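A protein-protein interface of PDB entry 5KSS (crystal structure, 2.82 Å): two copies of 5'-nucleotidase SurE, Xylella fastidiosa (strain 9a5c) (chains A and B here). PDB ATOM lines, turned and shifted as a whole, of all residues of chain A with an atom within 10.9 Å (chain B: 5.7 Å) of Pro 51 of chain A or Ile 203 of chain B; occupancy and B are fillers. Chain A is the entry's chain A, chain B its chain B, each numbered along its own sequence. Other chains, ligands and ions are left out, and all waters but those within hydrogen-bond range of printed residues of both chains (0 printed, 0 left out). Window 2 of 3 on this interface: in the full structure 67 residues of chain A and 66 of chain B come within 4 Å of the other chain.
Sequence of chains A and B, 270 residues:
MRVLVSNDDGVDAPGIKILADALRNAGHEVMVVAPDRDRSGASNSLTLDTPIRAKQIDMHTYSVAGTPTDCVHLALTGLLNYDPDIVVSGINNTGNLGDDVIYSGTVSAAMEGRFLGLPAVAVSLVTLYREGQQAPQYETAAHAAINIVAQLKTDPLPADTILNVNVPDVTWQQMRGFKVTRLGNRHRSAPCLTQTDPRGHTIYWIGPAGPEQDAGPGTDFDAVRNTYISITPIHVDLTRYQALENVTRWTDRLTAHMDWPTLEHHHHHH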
ATOM      1  N   ASP A  36      21.051 -23.067   3.880  1.00  0.00           N
ATOM      2  CA  ASP A  36      21.802 -23.999   3.049  1.00  0.00           C
ATOM      3  C   ASP A  36      22.334 -23.315   1.794  1.00  0.00           C
ATOM      4  O   ASP A  36      23.366 -23.707   1.250  1.00  0.00           O
ATOM      5  CB  ASP A  36      20.933 -25.201   2.668  1.00  0.00           C
ATOM      6  CG  ASP A  36      19.698 -24.801   1.884  1.00  0.00           C
ATOM      7  OD1 ASP A  36      19.205 -23.670   2.081  1.00  0.00           O
ATOM      8  OD2 ASP A  36      19.221 -25.619   1.071  1.00  0.00           O
ATOM      9  N   ARG A  39      19.836 -17.257   0.068  1.00  0.00           N
ATOM     10  CA  ARG A  39      18.406 -17.047  -0.126  1.00  0.00           C
ATOM     11  C   ARG A  39      18.044 -15.575  -0.303  1.00  0.00           C
ATOM     12  O   ARG A  39      16.910 -15.171  -0.044  1.00  0.00           O
ATOM     13  CB  ARG A  39      17.614 -17.653   1.033  1.00  0.00           C
ATOM     14  CG  ARG A  39      17.934 -19.113   1.291  1.00  0.00           C
ATOM     15  CD  ARG A  39      16.986 -19.710   2.310  1.00  0.00           C
ATOM     16  NE  ARG A  39      15.667 -19.980   1.746  1.00  0.00           N
ATOM     17  CZ  ARG A  39      15.317 -21.137   1.194  1.00  0.00           C
ATOM     18  NH1 ARG A  39      16.191 -22.133   1.131  1.00  0.00           N
ATOM     19  NH2 ARG A  39      14.096 -21.301   0.705  1.00  0.00           N
ATOM     20  N   LEU A  46       8.859 -16.571   8.540  1.00  0.00           N
ATOM     21  CA  LEU A  46       9.027 -17.878   9.160  1.00  0.00           C
ATOM     22  C   LEU A  46       8.283 -18.935   8.359  1.00  0.00           C
ATOM     23  O   LEU A  46       7.108 -18.766   8.031  1.00  0.00           O
ATOM     24  CB  LEU A  46       8.519 -17.864  10.603  1.00  0.00           C
ATOM     25  CG  LEU A  46       9.428 -17.215  11.646  1.00  0.00           C
ATOM     26  CD1 LEU A  46       8.761 -17.208  13.009  1.00  0.00           C
ATOM     27  CD2 LEU A  46      10.760 -17.941  11.705  1.00  0.00           C
ATOM     28  N   THR A  47       8.973 -20.025   8.041  1.00  0.00           N
ATOM     29  CA  THR A  47       8.354 -21.130   7.325  1.00  0.00           C
ATOM     30  C   THR A  47       7.423 -21.893   8.257  1.00  0.00           C
ATOM     31  O   THR A  47       7.875 -22.627   9.135  1.00  0.00           O
ATOM     32  CB  THR A  47       9.406 -22.093   6.756  1.00  0.00           C
ATOM     33  OG1 THR A  47      10.340 -21.364   5.947  1.00  0.00           O
ATOM     34  CG2 THR A  47       8.742 -23.160   5.911  1.00  0.00           C
ATOM     35  N   LEU A  48       6.121 -21.715   8.064  1.00  0.00           N
ATOM     36  CA  LEU A  48       5.133 -22.329   8.941  1.00  0.00           C
ATOM     37  C   LEU A  48       4.394 -23.473   8.257  1.00  0.00           C
ATOM     38  O   LEU A  48       4.044 -24.466   8.895  1.00  0.00           O
ATOM     39  CB  LEU A  48       4.132 -21.279   9.429  1.00  0.00           C
ATOM     40  CG  LEU A  48       4.722 -20.061  10.140  1.00  0.00           C
ATOM     41  CD1 LEU A  48       3.618 -19.126  10.610  1.00  0.00           C
ATOM     42  CD2 LEU A  48       5.601 -20.487  11.305  1.00  0.00           C
ATOM     43  N   ASP A  49       4.162 -23.331   6.956  1.00  0.00           N
ATOM     44  CA  ASP A  49       3.369 -24.304   6.209  1.00  0.00           C
ATOM     45  C   ASP A  49       4.105 -25.621   5.970  1.00  0.00           C
ATOM     46  O   ASP A  49       3.482 -26.683   5.914  1.00  0.00           O
ATOM     47  CB  ASP A  49       2.897 -23.708   4.879  1.00  0.00           C
ATOM     48  CG  ASP A  49       1.952 -22.536   5.070  1.00  0.00           C
ATOM     49  OD1 ASP A  49       1.331 -22.442   6.150  1.00  0.00           O
ATOM     50  OD2 ASP A  49       1.824 -21.714   4.138  1.00  0.00           O
ATOM     51  N   THR A  50       5.424 -25.551   5.830  1.00  0.00           N
ATOM     52  CA  THR A  50       6.232 -26.745   5.597  1.00  0.00           C
ATOM     53  C   THR A  50       7.284 -26.926   6.692  1.00  0.00           C
ATOM     54  O   THR A  50       7.707 -25.952   7.313  1.00  0.00           O
ATOM     55  CB  THR A  50       6.924 -26.702   4.213  1.00  0.00           C
ATOM     56  OG1 THR A  50       7.837 -25.601   4.158  1.00  0.00           O
ATOM     57  CG2 THR A  50       5.896 -26.558   3.103  1.00  0.00           C
ATOM     58  N   PRO A  51       7.700 -28.180   6.943  1.00  0.00           N
ATOM     59  CA  PRO A  51       8.748 -28.443   7.932  1.00  0.00           C
ATOM     60  C   PRO A  51      10.127 -28.108   7.380  1.00  0.00           C
ATOM     61  O   PRO A  51      10.297 -27.997   6.166  1.00  0.00           O
ATOM     62  CB  PRO A  51       8.627 -29.948   8.171  1.00  0.00           C
ATOM     63  CG  PRO A  51       8.104 -30.479   6.890  1.00  0.00           C
ATOM     64  CD  PRO A  51       7.168 -29.427   6.366  1.00  0.00           C
ATOM     65  N   ILE A  52      11.103 -27.958   8.268  1.00  0.00           N
ATOM     66  CA  ILE A  52      12.433 -27.518   7.872  1.00  0.00           C
ATOM     67  C   ILE A  52      13.499 -28.565   8.179  1.00  0.00           C
ATOM     68  O   ILE A  52      13.551 -29.106   9.282  1.00  0.00           O
ATOM     69  CB  ILE A  52      12.805 -26.205   8.581  1.00  0.00           C
ATOM     70  CG1 ILE A  52      11.667 -25.190   8.442  1.00  0.00           C
ATOM     71  CG2 ILE A  52      14.100 -25.648   8.022  1.00  0.00           C
ATOM     72  CD1 ILE A  52      11.798 -23.996   9.354  1.00  0.00           C
ATOM     73  N   ARG A  53      14.348 -28.846   7.195  1.00  0.00           N
ATOM     74  CA  ARG A  53      15.465 -29.763   7.388  1.00  0.00           C
ATOM     75  C   ARG A  53      16.676 -29.019   7.934  1.00  0.00           C
ATOM     76  O   ARG A  53      16.967 -27.898   7.515  1.00  0.00           O
ATOM     77  CB  ARG A  53      15.832 -30.457   6.075  1.00  0.00           C
ATOM     78  CG  ARG A  53      14.741 -31.349   5.508  1.00  0.00           C
ATOM     79  CD  ARG A  53      15.257 -32.151   4.324  1.00  0.00           C
ATOM     80  NE  ARG A  53      14.219 -32.996   3.738  1.00  0.00           N
ATOM     81  CZ  ARG A  53      13.950 -34.235   4.135  1.00  0.00           C
ATOM     82  NH1 ARG A  53      14.642 -34.781   5.127  1.00  0.00           N
ATOM     83  NH2 ARG A  53      12.989 -34.929   3.542  1.00  0.00           N
ATOM     84  N   ALA A  54      17.379 -29.644   8.872  1.00  0.00           N
ATOM     85  CA  ALA A  54      18.571 -29.040   9.452  1.00  0.00           C
ATOM     86  C   ALA A  54      19.726 -30.031   9.517  1.00  0.00           C
ATOM     87  O   ALA A  54      19.873 -30.765  10.492  1.00  0.00           O
ATOM     88  CB  ALA A  54      18.270 -28.480  10.830  1.00  0.00           C
ATOM     89  N   LYS A  55      20.538 -30.049   8.467  1.00  0.00           N
ATOM     90  CA  LYS A  55      21.720 -30.897   8.429  1.00  0.00           C
ATOM     91  C   LYS A  55      22.869 -30.223   9.173  1.00  0.00           C
ATOM     92  O   LYS A  55      23.066 -29.014   9.062  1.00  0.00           O
ATOM     93  CB  LYS A  55      22.126 -31.191   6.984  1.00  0.00           C
ATOM     94  N   GLN A  56      23.620 -31.009   9.936  1.00  0.00           N
ATOM     95  CA  GLN A  56      24.761 -30.483  10.671  1.00  0.00           C
ATOM     96  C   GLN A  56      26.057 -30.721   9.904  1.00  0.00           C
ATOM     97  O   GLN A  56      26.342 -31.844   9.487  1.00  0.00           O
ATOM     98  CB  GLN A  56      24.846 -31.120  12.059  1.00  0.00           C
ATOM     99  CG  GLN A  56      26.007 -30.614  12.895  1.00  0.00           C
ATOM    100  CD  GLN A  56      25.986 -31.155  14.311  1.00  0.00           C
ATOM    101  OE1 GLN A  56      25.204 -32.046  14.637  1.00  0.00           O
ATOM    102  NE2 GLN A  56      26.848 -30.611  15.162  1.00  0.00           N
ATOM    103  N   SER A  63      23.453 -26.520   9.013  1.00  0.00           N
ATOM    104  CA  SER A  63      22.916 -25.997   7.761  1.00  0.00           C
ATOM    105  C   SER A  63      21.404 -26.185   7.724  1.00  0.00           C
ATOM    106  O   SER A  63      20.897 -27.266   8.022  1.00  0.00           O
ATOM    107  CB  SER A  63      23.567 -26.689   6.564  1.00  0.00           C
ATOM    108  OG  SER A  63      23.146 -26.102   5.346  1.00  0.00           O
ATOM    109  N   VAL A  64      20.687 -25.130   7.353  1.00  0.00           N
ATOM    110  CA  VAL A  64      19.229 -25.137   7.410  1.00  0.00           C
ATOM    111  C   VAL A  64      18.589 -24.808   6.064  1.00  0.00           C
ATOM    112  O   VAL A  64      18.799 -23.729   5.512  1.00  0.00           O
ATOM    113  CB  VAL A  64      18.717 -24.150   8.477  1.00  0.00           C
ATOM    114  CG1 VAL A  64      17.227 -23.908   8.322  1.00  0.00           C
ATOM    115  CG2 VAL A  64      19.042 -24.663   9.870  1.00  0.00           C
ATOM    116  N   ALA A  65      17.802 -25.744   5.543  1.00  0.00           N
ATOM    117  CA  ALA A  65      17.091 -25.538   4.286  1.00  0.00           C
ATOM    118  C   ALA A  65      15.878 -24.637   4.498  1.00  0.00           C
ATOM    119  O   ALA A  65      14.738 -25.095   4.446  1.00  0.00           O
ATOM    120  CB  ALA A  65      16.666 -26.873   3.692  1.00  0.00           C
ATOM    121  N   GLY A  66      16.134 -23.355   4.738  1.00  0.00           N
ATOM    122  CA  GLY A  66      15.072 -22.402   4.998  1.00  0.00           C
ATOM    123  C   GLY A  66      15.592 -20.996   5.237  1.00  0.00           C
ATOM    124  O   GLY A  66      16.801 -20.763   5.241  1.00  0.00           O
ATOM    125  N   THR A  67      14.668 -20.063   5.449  1.00  0.00           N
ATOM    126  CA  THR A  67      14.995 -18.647   5.614  1.00  0.00           C
ATOM    127  C   THR A  67      15.889 -18.392   6.830  1.00  0.00           C
ATOM    128  O   THR A  67      15.915 -19.197   7.762  1.00  0.00           O
ATOM    129  CB  THR A  67      13.708 -17.800   5.738  1.00  0.00           C
ATOM    130  OG1 THR A  67      13.127 -17.990   7.034  1.00  0.00           O
ATOM    131  CG2 THR A  67      12.704 -18.199   4.669  1.00  0.00           C
ATOM    132  N   ASP A  70      14.104 -18.670   9.955  1.00  0.00           N
ATOM    133  CA  ASP A  70      13.902 -20.067  10.318  1.00  0.00           C
ATOM    134  C   ASP A  70      15.129 -20.606  11.037  1.00  0.00           C
ATOM    135  O   ASP A  70      15.016 -21.392  11.976  1.00  0.00           O
ATOM    136  CB  ASP A  70      13.614 -20.912   9.078  1.00  0.00           C
ATOM    137  CG  ASP A  70      12.316 -20.527   8.399  1.00  0.00           C
ATOM    138  OD1 ASP A  70      11.369 -20.127   9.107  1.00  0.00           O
ATOM    139  OD2 ASP A  70      12.245 -20.621   7.156  1.00  0.00           O
ATOM    140  N   CYS A  71      16.304 -20.176  10.587  1.00  0.00           N
ATOM    141  CA  CYS A  71      17.559 -20.581  11.206  1.00  0.00           C
ATOM    142  C   CYS A  71      17.600 -20.165  12.671  1.00  0.00           C
ATOM    143  O   CYS A  71      17.766 -21.001  13.558  1.00  0.00           O
ATOM    144  CB  CYS A  71      18.746 -19.971  10.459  1.00  0.00           C
ATOM    145  SG  CYS A  71      18.945 -20.551   8.766  1.00  0.00           S
ATOM    146  N   LEU A  74      14.504 -21.675  14.960  1.00  0.00           N
ATOM    147  CA  LEU A  74      14.725 -23.069  15.329  1.00  0.00           C
ATOM    148  C   LEU A  74      15.873 -23.204  16.322  1.00  0.00           C
ATOM    149  O   LEU A  74      15.772 -23.943  17.301  1.00  0.00           O
ATOM    150  CB  LEU A  74      14.994 -23.926  14.089  1.00  0.00           C
ATOM    151  CG  LEU A  74      13.824 -24.122  13.121  1.00  0.00           C
ATOM    152  CD1 LEU A  74      14.185 -25.133  12.043  1.00  0.00           C
ATOM    153  CD2 LEU A  74      12.568 -24.550  13.864  1.00  0.00           C
ATOM    154  N   GLY A  78      14.529 -25.300  20.258  1.00  0.00           N
ATOM    155  CA  GLY A  78      14.620 -26.742  20.415  1.00  0.00           C
ATOM    156  C   GLY A  78      15.705 -27.424  19.605  1.00  0.00           C
ATOM    157  O   GLY A  78      16.175 -28.500  19.980  1.00  0.00           O
ATOM    158  N   LEU A  79      16.097 -26.810  18.492  1.00  0.00           N
ATOM    159  CA  LEU A  79      17.144 -27.363  17.636  1.00  0.00           C
ATOM    160  C   LEU A  79      18.457 -27.505  18.398  1.00  0.00           C
ATOM    161  O   LEU A  79      19.222 -28.440  18.168  1.00  0.00           O
ATOM    162  CB  LEU A  79      17.336 -26.488  16.389  1.00  0.00           C
ATOM    163  CG  LEU A  79      18.667 -26.494  15.626  1.00  0.00           C
ATOM    164  CD1 LEU A  79      18.995 -27.862  15.046  1.00  0.00           C
ATOM    165  CD2 LEU A  79      18.647 -25.445  14.524  1.00  0.00           C
ATOM    166  N   LEU B 193       8.915 -28.560  17.087  1.00  0.00           N
ATOM    167  CA  LEU B 193       8.672 -29.991  17.222  1.00  0.00           C
ATOM    168  C   LEU B 193       9.517 -30.792  16.237  1.00  0.00           C
ATOM    169  O   LEU B 193       9.844 -30.311  15.153  1.00  0.00           O
ATOM    170  CB  LEU B 193       7.187 -30.299  17.018  1.00  0.00           C
ATOM    171  CG  LEU B 193       6.227 -29.629  18.002  1.00  0.00           C
ATOM    172  CD1 LEU B 193       4.812 -30.158  17.815  1.00  0.00           C
ATOM    173  CD2 LEU B 193       6.697 -29.829  19.437  1.00  0.00           C
ATOM    174  N   THR B 194       9.863 -32.014  16.620  1.00  0.00           N
ATOM    175  CA  THR B 194      10.731 -32.854  15.806  1.00  0.00           C
ATOM    176  C   THR B 194      10.045 -34.146  15.370  1.00  0.00           C
ATOM    177  O   THR B 194       9.769 -35.023  16.189  1.00  0.00           O
ATOM    178  CB  THR B 194      12.030 -33.203  16.554  1.00  0.00           C
ATOM    179  OG1 THR B 194      12.795 -32.011  16.769  1.00  0.00           O
ATOM    180  CG2 THR B 194      12.860 -34.187  15.750  1.00  0.00           C
ATOM    181  N   GLN B 195       9.774 -34.251  14.073  1.00  0.00           N
ATOM    182  CA  GLN B 195       9.204 -35.458  13.490  1.00  0.00           C
ATOM    183  C   GLN B 195      10.176 -36.027  12.465  1.00  0.00           C
ATOM    184  O   GLN B 195      11.266 -35.491  12.268  1.00  0.00           O
ATOM    185  CB  GLN B 195       7.879 -35.136  12.798  1.00  0.00           C
ATOM    186  CG  GLN B 195       6.894 -34.359  13.652  1.00  0.00           C
ATOM    187  CD  GLN B 195       5.687 -33.890  12.863  1.00  0.00           C
ATOM    188  OE1 GLN B 195       5.640 -34.023  11.639  1.00  0.00           O
ATOM    189  NE2 GLN B 195       4.702 -33.335  13.560  1.00  0.00           N
ATOM    190  N   THR B 196       9.775 -37.109  11.804  1.00  0.00           N
ATOM    191  CA  THR B 196      10.603 -37.716  10.769  1.00  0.00           C
ATOM    192  C   THR B 196       9.839 -37.862   9.457  1.00  0.00           C
ATOM    193  O   THR B 196       8.628 -38.075   9.453  1.00  0.00           O
ATOM    194  CB  THR B 196      11.128 -39.101  11.198  1.00  0.00           C
ATOM    195  OG1 THR B 196      10.024 -39.959  11.513  1.00  0.00           O
ATOM    196  CG2 THR B 196      12.034 -38.979  12.415  1.00  0.00           C
ATOM    197  N   ASP B 197      10.556 -37.735   8.346  1.00  0.00           N
ATOM    198  CA  ASP B 197       9.977 -37.959   7.029  1.00  0.00           C
ATOM    199  C   ASP B 197       9.881 -39.462   6.765  1.00  0.00           C
ATOM    200  O   ASP B 197      10.480 -40.252   7.494  1.00  0.00           O
ATOM    201  CB  ASP B 197      10.811 -37.253   5.950  1.00  0.00           C
ATOM    202  CG  ASP B 197      12.295 -37.560   6.053  1.00  0.00           C
ATOM    203  OD1 ASP B 197      12.659 -38.737   6.253  1.00  0.00           O
ATOM    204  OD2 ASP B 197      13.102 -36.615   5.932  1.00  0.00           O
ATOM    205  N   HIS B 201      14.741 -39.308   7.713  1.00  0.00           N
ATOM    206  CA  HIS B 201      15.590 -38.163   8.026  1.00  0.00           C
ATOM    207  C   HIS B 201      14.858 -37.159   8.909  1.00  0.00           C
ATOM    208  O   HIS B 201      13.655 -36.949   8.768  1.00  0.00           O
ATOM    209  CB  HIS B 201      16.101 -37.496   6.750  1.00  0.00           C
ATOM    210  CG  HIS B 201      17.120 -38.310   6.015  1.00  0.00           C
ATOM    211  ND1 HIS B 201      18.461 -38.287   6.334  1.00  0.00           N
ATOM    212  CD2 HIS B 201      16.996 -39.173   4.980  1.00  0.00           C
ATOM    213  CE1 HIS B 201      19.118 -39.099   5.526  1.00  0.00           C
ATOM    214  NE2 HIS B 201      18.252 -39.649   4.695  1.00  0.00           N
ATOM    215  N   THR B 202      15.601 -36.543   9.820  1.00  0.00           N
ATOM    216  CA  THR B 202      15.015 -35.693  10.845  1.00  0.00           C
ATOM    217  C   THR B 202      14.603 -34.325  10.303  1.00  0.00           C
ATOM    218  O   THR B 202      15.433 -33.574   9.791  1.00  0.00           O
ATOM    219  CB  THR B 202      15.987 -35.517  12.028  1.00  0.00           C
ATOM    220  OG1 THR B 202      16.502 -36.797  12.417  1.00  0.00           O
ATOM    221  CG2 THR B 202      15.284 -34.882  13.208  1.00  0.00           C
ATOM    222  N   ILE B 203      13.314 -34.012  10.413  1.00  0.00           N
ATOM    223  CA  ILE B 203      12.788 -32.720   9.983  1.00  0.00           C
ATOM    224  C   ILE B 203      12.214 -31.938  11.163  1.00  0.00           C
ATOM    225  O   ILE B 203      11.768 -32.523  12.150  1.00  0.00           O
ATOM    226  CB  ILE B 203      11.698 -32.874   8.903  1.00  0.00           C
ATOM    227  CG1 ILE B 203      10.523 -33.695   9.441  1.00  0.00           C
ATOM    228  CG2 ILE B 203      12.276 -33.512   7.649  1.00  0.00           C
ATOM    229  CD1 ILE B 203       9.409 -33.902   8.441  1.00  0.00           C
ATOM    230  N   TYR B 204      12.228 -30.611  11.056  1.00  0.00           N
ATOM    231  CA  TYR B 204      11.783 -29.749  12.147  1.00  0.00           C
ATOM    232  C   TYR B 204      10.574 -28.895  11.771  1.00  0.00           C
ATOM    233  O   TYR B 204      10.556 -28.246  10.725  1.00  0.00           O
ATOM    234  CB  TYR B 204      12.922 -28.834  12.610  1.00  0.00           C
ATOM    235  CG  TYR B 204      14.148 -29.562  13.111  1.00  0.00           C
ATOM    236  CD1 TYR B 204      14.057 -30.845  13.634  1.00  0.00           C
ATOM    237  CD2 TYR B 204      15.399 -28.962  13.065  1.00  0.00           C
ATOM    238  CE1 TYR B 204      15.176 -31.511  14.094  1.00  0.00           C
ATOM    239  CE2 TYR B 204      16.522 -29.623  13.523  1.00  0.00           C
ATOM    240  CZ  TYR B 204      16.407 -30.895  14.034  1.00  0.00           C
ATOM    241  OH  TYR B 204      17.526 -31.554  14.489  1.00  0.00           O
ATOM    242  N   TRP B 205       9.567 -28.898  12.638  1.00  0.00           N
ATOM    243  CA  TRP B 205       8.407 -28.029  12.474  1.00  0.00           C
ATOM    244  C   TRP B 205       8.518 -26.834  13.410  1.00  0.00           C
ATOM    245  O   TRP B 205       8.849 -26.994  14.585  1.00  0.00           O
ATOM    246  CB  TRP B 205       7.121 -28.790  12.790  1.00  0.00           C
ATOM    247  CG  TRP B 205       6.603 -29.639  11.673  1.00  0.00           C
ATOM    248  CD1 TRP B 205       6.795 -30.980  11.504  1.00  0.00           C
ATOM    249  CD2 TRP B 205       5.791 -29.209  10.576  1.00  0.00           C
ATOM    250  NE1 TRP B 205       6.155 -31.409  10.366  1.00  0.00           N
ATOM    251  CE2 TRP B 205       5.531 -30.339   9.778  1.00  0.00           C
ATOM    252  CE3 TRP B 205       5.261 -27.973  10.188  1.00  0.00           C
ATOM    253  CZ2 TRP B 205       4.764 -30.274   8.618  1.00  0.00           C
ATOM    254  CZ3 TRP B 205       4.501 -27.910   9.036  1.00  0.00           C
ATOM    255  CH2 TRP B 205       4.260 -29.052   8.264  1.00  0.00           C
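NH1 of Arg 53 of chain A is in salt-bridge range of OD2 of Asp 197 of chain B. The backbone carbonyl oxygen (O) of Tyr 204 of chain B lies within hydrogen-bond range of the backbone NH (N) of Ile 52 of chain A (2.5 Å).
O of Arg 53 of chain A lies within hydrogen-bond range of N of Ala 65 of chain A (3.0 Å). N of Ile 203 of chain B lies within hydrogen-bond range of O of Gln 195 of chain B (3.1 Å). The backbone NH (N) of Trp 205 of chain B sits at hydrogen-bond distance from the backbone carbonyl oxygen (O) of Leu 193 of chain B, 2.9 Å away. O of Leu 74 of chain A sits at hydrogen-bond distance from N of Leu 79 of chain A (3.1 Å). OD1 of Asp 197 of chain B lies within hydrogen-bond range of N of His 201 of chain B, 2.6 Å away. NE1 of Trp 205 of chain B is in hydrogen-bond range of OE1 of Gln 195 of chain B.
O of Leu 48 of chain A touches CZ3 of Trp 205 of chain B, 3.5 Å away. O of Asp 49 of chain A touches CH2 of Trp 205 of chain B, at 3.4 Å. Thr 50 of chain A touches Trp 205 of chain B. Ile 203 of chain B touches Pro 51 of chain A (CD1 to CG, 3.98 Å). Tyr 204 of chain B touches Pro 51 of chain A. Pro 51 of chain A touches Trp 205 of chain B (CD to CZ2, 3.4 Å). C of Ile 203 of chain B touches O of Ile 52 of chain A (3.7 Å). CB of His 201 of chain B touches NH1 of Arg 53 of chain A (3.5 Å). CD1 of Leu 74 of chain A touches CB of Tyr 204 of chain B, at 3.95 Å. Tyr 204 of chain B touches Leu 79 of chain A (CE2 to CD1, 3.4 Å).
Of the printed residues of chain B, Asp 49 of chain A touches Trp 205. Of chain B, only Ile 203, Tyr 204 and Trp 205 come within 4 Å of Pro 51 of chain A. Of the printed residues of chain B, Arg 53 of chain A touches Asp 197 (2.5 Å), His 201 (3.5 Å) and Ile 203 (3.7 Å). Thr 67 of chain A touches none of the printed residues of chain B. Gly 78 of chain A touches none of the printed residues of chain B. No residue of chain A comes within 4 Å of Thr 194 of chain B. Of chain A, only Arg 53 (2.5 Å) comes within 4 Å of Asp 197 of chain B. Of chain A, only Leu 48 (3.5 Å), Asp 49 (3.4 Å), Thr 50 (3.8 Å) and Pro 51 (3.4 Å) come within 4 Å of Trp 205 of chain B. The nearest printed residue of chain B that does not touch Pro 51 of chain A is Gln 195 of chain B (6.1 Å).
Printed residues of chain A that touch a printed residue of chain B: Leu 48, Asp 49, Thr 50, Pro 51, Ile 52, Arg 53, Ala 54, Leu 74 and Leu 79. Hydrophobic or aromatic side chains of chain A within 4 Å of the printed part of chain B: Pro 51, Ile 52, Ala 54, Leu 74 and Leu 79. Of the 10 printed residues of chain B, 5 touch a printed residue of chain A. Hydrophobic or aromatic side chains of chain B within 4 Å of the printed part of chain A: His 201, Ile 203, Tyr 204 and Trp 205. Among the printed residues, 14 pairs touch across the chains.
No position is printed for both chains. Of the 14 pairs that touch across the chains among the printed residues, none has its exchanged pair printed and touching as well.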
